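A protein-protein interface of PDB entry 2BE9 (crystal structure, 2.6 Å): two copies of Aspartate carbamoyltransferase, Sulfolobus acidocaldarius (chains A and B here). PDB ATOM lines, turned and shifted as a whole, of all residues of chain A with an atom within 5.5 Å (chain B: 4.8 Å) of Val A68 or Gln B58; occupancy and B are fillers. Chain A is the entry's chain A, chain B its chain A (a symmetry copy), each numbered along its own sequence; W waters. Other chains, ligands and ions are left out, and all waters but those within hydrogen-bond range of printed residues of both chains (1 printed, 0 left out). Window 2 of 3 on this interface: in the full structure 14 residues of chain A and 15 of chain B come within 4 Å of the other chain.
Val A68 touches Gln B58, but with the chains exchanged Gln A58 does not touch Val B68 (9.4 Å). Of the 6 pairs that touch across the chains among the printed residues, none has its exchanged pair printed and touching as well.
Hydrophobic or aromatic side chains of chain B within 4 Å of the printed part of chain A: Leu B55 and Ile B62. Of the 12 printed residues of chain A, 5 touch a printed residue of chain B. Printed residues of chain A that touch a printed residue of chain B: Thr A41, Asp A67, Val A68, Ile A69 and Gly A70. Among the printed residues, 6 pairs touch across the chains.
N of Ile A44 lies within hydrogen-bond range of O of Ile A69, 2.8 Å away. The backbone carbonyl oxygen (O) of Ile A42 lies within hydrogen-bond range of the backbone NH (N) of Ile A69 (3.3 Å). The backbone NH of Ile A42 lies within hydrogen-bond range of the backbone carbonyl oxygen of Asp A67 (2.9 Å).
Water W1 bridges N of Gly A70 and NE2 of Gln B58.
Among the printed residues, pairs that only touch across the chains: Thr A41 with Lys B59, Ile A69 with Gln B58, Val A68 with Gln B58, Gly A70 with Leu B55, Asp A67 with Ile B62 and Ile A69 with Ile B62.
Of the printed residues of chain B, Thr A41 touches Lys B59. Of chain B, only Gln B58 comes within 4 Å of Val A68. Of the printed residues of chain B, Ile A69 touches Gln B58 and Ile B62. Tyr B54 touches none of the printed residues of chain A. Printed residues of chain A within 4 Å of Leu B55: Gly A70. Gln B58 touches two residues of chain A. Of the printed residues of chain A, Lys B59 touches Thr A41 (3.2 Å). Ile B61 touches none of the printed residues of chain A. Of the printed residues of chain A, Ile B62 touches Asp A67 and Ile A69. The nearest printed residue of chain B that does not touch Asp A67 is Lys B59 (6.3 Å).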
ATOM      1  N   THR A  41      -8.070 -33.853   4.870  1.00  0.00           N
ATOM      2  CA  THR A  41      -7.319 -32.809   5.546  1.00  0.00           C
ATOM      3  C   THR A  41      -5.895 -32.827   5.024  1.00  0.00           C
ATOM      4  O   THR A  41      -5.205 -33.849   5.116  1.00  0.00           O
ATOM      5  CB  THR A  41      -7.378 -32.951   7.092  1.00  0.00           C
ATOM      6  OG1 THR A  41      -8.745 -32.807   7.549  1.00  0.00           O
ATOM      7  CG2 THR A  41      -6.492 -31.907   7.790  1.00  0.00           C
ATOM      8  N   ILE A  42      -5.471 -31.716   4.432  1.00  0.00           N
ATOM      9  CA  ILE A  42      -4.057 -31.533   4.084  1.00  0.00           C
ATOM     10  C   ILE A  42      -3.337 -30.704   5.146  1.00  0.00           C
ATOM     11  O   ILE A  42      -3.839 -29.634   5.542  1.00  0.00           O
ATOM     12  CB  ILE A  42      -3.887 -30.856   2.735  1.00  0.00           C
ATOM     13  CG1 ILE A  42      -4.656 -31.634   1.658  1.00  0.00           C
ATOM     14  CG2 ILE A  42      -2.404 -30.739   2.402  1.00  0.00           C
ATOM     15  CD1 ILE A  42      -4.298 -33.127   1.566  1.00  0.00           C
ATOM     16  N   ILE A  44      -0.170 -28.351   6.197  1.00  0.00           N
ATOM     17  CA  ILE A  44       0.833 -27.448   5.622  1.00  0.00           C
ATOM     18  C   ILE A  44       1.896 -27.181   6.677  1.00  0.00           C
ATOM     19  O   ILE A  44       1.690 -26.420   7.618  1.00  0.00           O
ATOM     20  CB  ILE A  44       0.183 -26.161   5.063  1.00  0.00           C
ATOM     21  CG1 ILE A  44      -0.913 -26.523   4.054  1.00  0.00           C
ATOM     22  CG2 ILE A  44       1.220 -25.276   4.373  1.00  0.00           C
ATOM     23  CD1 ILE A  44      -1.710 -25.330   3.558  1.00  0.00           C
ATOM     24  N   TYR A  54       2.672 -20.630   1.429  1.00  0.00           N
ATOM     25  CA  TYR A  54       1.708 -21.165   2.369  1.00  0.00           C
ATOM     26  C   TYR A  54       0.264 -20.928   1.851  1.00  0.00           C
ATOM     27  O   TYR A  54      -0.542 -21.853   1.752  1.00  0.00           O
ATOM     28  CB  TYR A  54       1.927 -20.531   3.757  1.00  0.00           C
ATOM     29  CG  TYR A  54       1.211 -21.269   4.856  1.00  0.00           C
ATOM     30  CD1 TYR A  54      -0.183 -21.199   4.993  1.00  0.00           C
ATOM     31  CD2 TYR A  54       1.909 -22.067   5.737  1.00  0.00           C
ATOM     32  CE1 TYR A  54      -0.864 -21.928   6.013  1.00  0.00           C
ATOM     33  CE2 TYR A  54       1.257 -22.782   6.753  1.00  0.00           C
ATOM     34  CZ  TYR A  54      -0.127 -22.718   6.890  1.00  0.00           C
ATOM     35  OH  TYR A  54      -0.745 -23.440   7.899  1.00  0.00           O
ATOM     36  N   GLN A  58      -2.853 -23.350   0.560  1.00  0.00           N
ATOM     37  CA  GLN A  58      -4.069 -23.326   1.333  1.00  0.00           C
ATOM     38  C   GLN A  58      -5.259 -22.994   0.438  1.00  0.00           C
ATOM     39  O   GLN A  58      -6.275 -23.685   0.478  1.00  0.00           O
ATOM     40  CB  GLN A  58      -3.942 -22.313   2.451  1.00  0.00           C
ATOM     41  CG  GLN A  58      -5.103 -22.336   3.384  1.00  0.00           C
ATOM     42  CD  GLN A  58      -4.897 -21.428   4.583  1.00  0.00           C
ATOM     43  OE1 GLN A  58      -5.748 -21.383   5.488  1.00  0.00           O
ATOM     44  NE2 GLN A  58      -3.772 -20.697   4.601  1.00  0.00           N
ATOM     45  N   ILE A  61      -6.118 -25.855  -1.763  1.00  0.00           N
ATOM     46  CA  ILE A  61      -6.820 -26.891  -1.023  1.00  0.00           C
ATOM     47  C   ILE A  61      -8.285 -26.510  -0.710  1.00  0.00           C
ATOM     48  O   ILE A  61      -9.204 -27.328  -0.888  1.00  0.00           O
ATOM     49  CB  ILE A  61      -6.068 -27.283   0.242  1.00  0.00           C
ATOM     50  CG1 ILE A  61      -4.716 -27.876  -0.121  1.00  0.00           C
ATOM     51  CG2 ILE A  61      -6.880 -28.295   1.058  1.00  0.00           C
ATOM     52  CD1 ILE A  61      -3.673 -27.662   0.979  1.00  0.00           C
ATOM     53  N   ILE A  62      -8.489 -25.273  -0.253  1.00  0.00           N
ATOM     54  CA  ILE A  62      -9.826 -24.748   0.000  1.00  0.00           C
ATOM     55  C   ILE A  62     -10.706 -24.871  -1.256  1.00  0.00           C
ATOM     56  O   ILE A  62     -11.858 -25.319  -1.164  1.00  0.00           O
ATOM     57  CB  ILE A  62      -9.768 -23.282   0.535  1.00  0.00           C
ATOM     58  CG1 ILE A  62      -9.387 -23.279   2.025  1.00  0.00           C
ATOM     59  CG2 ILE A  62     -11.086 -22.515   0.286  1.00  0.00           C
ATOM     60  CD1 ILE A  62      -9.089 -21.863   2.589  1.00  0.00           C
ATOM     61  N   GLY A  66     -10.976 -29.305   0.514  1.00  0.00           N
ATOM     62  CA  GLY A  66     -10.178 -29.796   1.640  1.00  0.00           C
ATOM     63  C   GLY A  66     -10.186 -28.915   2.886  1.00  0.00           C
ATOM     64  O   GLY A  66     -10.409 -27.712   2.812  1.00  0.00           O
ATOM     65  N   ASP A  67      -9.955 -29.535   4.036  1.00  0.00           N
ATOM     66  CA  ASP A  67      -9.617 -28.836   5.282  1.00  0.00           C
ATOM     67  C   ASP A  67      -8.104 -28.674   5.433  1.00  0.00           C
ATOM     68  O   ASP A  67      -7.305 -29.531   5.000  1.00  0.00           O
ATOM     69  CB  ASP A  67     -10.164 -29.604   6.489  1.00  0.00           C
ATOM     70  CG  ASP A  67     -11.674 -29.701   6.456  1.00  0.00           C
ATOM     71  OD1 ASP A  67     -12.315 -28.627   6.510  1.00  0.00           O
ATOM     72  OD2 ASP A  67     -12.211 -30.829   6.330  1.00  0.00           O
ATOM     73  N   VAL A  68      -7.731 -27.565   6.062  1.00  0.00           N
ATOM     74  CA  VAL A  68      -6.359 -27.191   6.241  1.00  0.00           C
ATOM     75  C   VAL A  68      -5.990 -27.107   7.718  1.00  0.00           C
ATOM     76  O   VAL A  68      -6.659 -26.418   8.494  1.00  0.00           O
ATOM     77  CB  VAL A  68      -6.073 -25.850   5.570  1.00  0.00           C
ATOM     78  CG1 VAL A  68      -4.611 -25.425   5.838  1.00  0.00           C
ATOM     79  CG2 VAL A  68      -6.328 -25.952   4.100  1.00  0.00           C
ATOM     80  N   ILE A  69      -4.934 -27.832   8.084  1.00  0.00           N
ATOM     81  CA  ILE A  69      -4.206 -27.621   9.326  1.00  0.00           C
ATOM     82  C   ILE A  69      -2.733 -27.369   8.967  1.00  0.00           C
ATOM     83  O   ILE A  69      -2.260 -27.732   7.880  1.00  0.00           O
ATOM     84  CB  ILE A  69      -4.303 -28.832  10.287  1.00  0.00           C
ATOM     85  CG1 ILE A  69      -3.734 -30.104   9.632  1.00  0.00           C
ATOM     86  CG2 ILE A  69      -5.736 -29.043  10.753  1.00  0.00           C
ATOM     87  CD1 ILE A  69      -3.499 -31.280  10.610  1.00  0.00           C
ATOM     88  N   GLY A  70      -1.993 -26.740   9.862  1.00  0.00           N
ATOM     89  CA  GLY A  70      -0.587 -26.566   9.597  1.00  0.00           C
ATOM     90  C   GLY A  70       0.097 -25.698  10.608  1.00  0.00           C
ATOM     91  O   GLY A  70      -0.480 -25.326  11.624  1.00  0.00           O
ATOM     92  N   ILE B  44      -8.796 -22.271  20.214  1.00  0.00           N
ATOM     93  CA  ILE B  44      -7.583 -22.950  20.683  1.00  0.00           C
ATOM     94  C   ILE B  44      -6.561 -21.889  21.067  1.00  0.00           C
ATOM     95  O   ILE B  44      -5.933 -21.266  20.216  1.00  0.00           O
ATOM     96  CB  ILE B  44      -7.059 -23.961  19.637  1.00  0.00           C
ATOM     97  CG1 ILE B  44      -8.167 -24.953  19.267  1.00  0.00           C
ATOM     98  CG2 ILE B  44      -5.858 -24.738  20.178  1.00  0.00           C
ATOM     99  CD1 ILE B  44      -7.793 -25.897  18.137  1.00  0.00           C
ATOM    100  N   TYR B  54      -1.839 -28.731  19.668  1.00  0.00           N
ATOM    101  CA  TYR B  54      -2.680 -27.817  18.924  1.00  0.00           C
ATOM    102  C   TYR B  54      -3.447 -28.579  17.809  1.00  0.00           C
ATOM    103  O   TYR B  54      -4.671 -28.501  17.704  1.00  0.00           O
ATOM    104  CB  TYR B  54      -1.823 -26.673  18.345  1.00  0.00           C
ATOM    105  CG  TYR B  54      -2.647 -25.512  17.858  1.00  0.00           C
ATOM    106  CD1 TYR B  54      -3.406 -25.599  16.682  1.00  0.00           C
ATOM    107  CD2 TYR B  54      -2.707 -24.341  18.582  1.00  0.00           C
ATOM    108  CE1 TYR B  54      -4.216 -24.511  16.242  1.00  0.00           C
ATOM    109  CE2 TYR B  54      -3.489 -23.255  18.158  1.00  0.00           C
ATOM    110  CZ  TYR B  54      -4.246 -23.341  16.993  1.00  0.00           C
ATOM    111  OH  TYR B  54      -5.015 -22.255  16.601  1.00  0.00           O
ATOM    112  N   LEU B  55      -2.697 -29.331  17.010  1.00  0.00           N
ATOM    113  CA  LEU B  55      -3.184 -29.940  15.797  1.00  0.00           C
ATOM    114  C   LEU B  55      -4.114 -31.090  16.114  1.00  0.00           C
ATOM    115  O   LEU B  55      -5.091 -31.329  15.409  1.00  0.00           O
ATOM    116  CB  LEU B  55      -2.008 -30.444  14.980  1.00  0.00           C
ATOM    117  CG  LEU B  55      -1.529 -29.596  13.808  1.00  0.00           C
ATOM    118  CD1 LEU B  55      -1.727 -28.106  13.984  1.00  0.00           C
ATOM    119  CD2 LEU B  55      -0.082 -29.948  13.520  1.00  0.00           C
ATOM    120  N   SER B  56      -3.797 -31.795  17.182  1.00  0.00           N
ATOM    121  CA  SER B  56      -4.615 -32.872  17.686  1.00  0.00           C
ATOM    122  C   SER B  56      -6.030 -32.376  17.998  1.00  0.00           C
ATOM    123  O   SER B  56      -7.026 -32.940  17.524  1.00  0.00           O
ATOM    124  CB  SER B  56      -3.962 -33.406  18.954  1.00  0.00           C
ATOM    125  OG  SER B  56      -4.822 -34.336  19.549  1.00  0.00           O
ATOM    126  N   PHE B  57      -6.124 -31.299  18.774  1.00  0.00           N
ATOM    127  CA  PHE B  57      -7.438 -30.774  19.103  1.00  0.00           C
ATOM    128  C   PHE B  57      -8.157 -30.218  17.877  1.00  0.00           C
ATOM    129  O   PHE B  57      -9.343 -30.459  17.674  1.00  0.00           O
ATOM    130  CB  PHE B  57      -7.333 -29.721  20.179  1.00  0.00           C
ATOM    131  CG  PHE B  57      -7.376 -30.278  21.570  1.00  0.00           C
ATOM    132  CD1 PHE B  57      -6.211 -30.336  22.344  1.00  0.00           C
ATOM    133  CD2 PHE B  57      -8.588 -30.717  22.121  1.00  0.00           C
ATOM    134  CE1 PHE B  57      -6.251 -30.828  23.646  1.00  0.00           C
ATOM    135  CE2 PHE B  57      -8.640 -31.208  23.411  1.00  0.00           C
ATOM    136  CZ  PHE B  57      -7.467 -31.268  24.182  1.00  0.00           C
ATOM    137  N   GLN B  58      -7.427 -29.486  17.044  1.00  0.00           N
ATOM    138  CA  GLN B  58      -8.009 -28.937  15.846  1.00  0.00           C
ATOM    139  C   GLN B  58      -8.612 -30.047  14.991  1.00  0.00           C
ATOM    140  O   GLN B  58      -9.756 -29.939  14.554  1.00  0.00           O
ATOM    141  CB  GLN B  58      -6.955 -28.177  15.070  1.00  0.00           C
ATOM    142  CG  GLN B  58      -7.514 -27.452  13.894  1.00  0.00           C
ATOM    143  CD  GLN B  58      -6.481 -26.574  13.213  1.00  0.00           C
ATOM    144  OE1 GLN B  58      -6.806 -25.854  12.253  1.00  0.00           O
ATOM    145  NE2 GLN B  58      -5.231 -26.625  13.698  1.00  0.00           N
ATOM    146  N   LYS B  59      -7.861 -31.127  14.781  1.00  0.00           N
ATOM    147  CA  LYS B  59      -8.368 -32.227  13.970  1.00  0.00           C
ATOM    148  C   LYS B  59      -9.627 -32.867  14.585  1.00  0.00           C
ATOM    149  O   LYS B  59     -10.622 -33.087  13.882  1.00  0.00           O
ATOM    150  CB  LYS B  59      -7.294 -33.287  13.689  1.00  0.00           C
ATOM    151  CG  LYS B  59      -7.772 -34.299  12.641  1.00  0.00           C
ATOM    152  CD  LYS B  59      -7.833 -33.637  11.264  1.00  0.00           C
ATOM    153  CE  LYS B  59      -8.715 -34.392  10.286  1.00  0.00           C
ATOM    154  NZ  LYS B  59      -8.400 -35.800  10.328  1.00  0.00           N
ATOM    155  N   ALA B  60      -9.555 -33.163  15.884  1.00  0.00           N
ATOM    156  CA  ALA B  60     -10.712 -33.567  16.675  1.00  0.00           C
ATOM    157  C   ALA B  60     -11.922 -32.676  16.402  1.00  0.00           C
ATOM    158  O   ALA B  60     -13.008 -33.169  16.072  1.00  0.00           O
ATOM    159  CB  ALA B  60     -10.371 -33.542  18.162  1.00  0.00           C
ATOM    160  N   ILE B  61     -11.732 -31.361  16.510  1.00  0.00           N
ATOM    161  CA  ILE B  61     -12.841 -30.445  16.301  1.00  0.00           C
ATOM    162  C   ILE B  61     -13.370 -30.472  14.849  1.00  0.00           C
ATOM    163  O   ILE B  61     -14.590 -30.517  14.620  1.00  0.00           O
ATOM    164  CB  ILE B  61     -12.486 -29.029  16.735  1.00  0.00           C
ATOM    165  CG1 ILE B  61     -12.200 -29.000  18.228  1.00  0.00           C
ATOM    166  CG2 ILE B  61     -13.630 -28.064  16.403  1.00  0.00           C
ATOM    167  CD1 ILE B  61     -11.224 -27.885  18.611  1.00  0.00           C
ATOM    168  N   ILE B  62     -12.448 -30.450  13.884  1.00  0.00           N
ATOM    169  CA  ILE B  62     -12.797 -30.559  12.472  1.00  0.00           C
ATOM    170  C   ILE B  62     -13.630 -31.826  12.214  1.00  0.00           C
ATOM    171  O   ILE B  62     -14.656 -31.764  11.522  1.00  0.00           O
ATOM    172  CB  ILE B  62     -11.526 -30.496  11.566  1.00  0.00           C
ATOM    173  CG1 ILE B  62     -11.048 -29.042  11.428  1.00  0.00           C
ATOM    174  CG2 ILE B  62     -11.758 -31.149  10.186  1.00  0.00           C
ATOM    175  CD1 ILE B  62      -9.668 -28.902  10.731  1.00  0.00           C
ATOM    176  N   VAL B  68     -12.739 -23.695  13.871  1.00  0.00           N
ATOM    177  CA  VAL B  68     -11.593 -23.450  14.697  1.00  0.00           C
ATOM    178  C   VAL B  68     -11.061 -22.034  14.508  1.00  0.00           C
ATOM    179  O   VAL B  68     -10.794 -21.607  13.381  1.00  0.00           O
ATOM    180  CB  VAL B  68     -10.484 -24.453  14.393  1.00  0.00           C
ATOM    181  CG1 VAL B  68      -9.230 -24.126  15.236  1.00  0.00           C
ATOM    182  CG2 VAL B  68     -10.961 -25.841  14.678  1.00  0.00           C
HETATM  183  O   HOH W   1      -3.414 -25.377  11.738  1.00  0.00           O
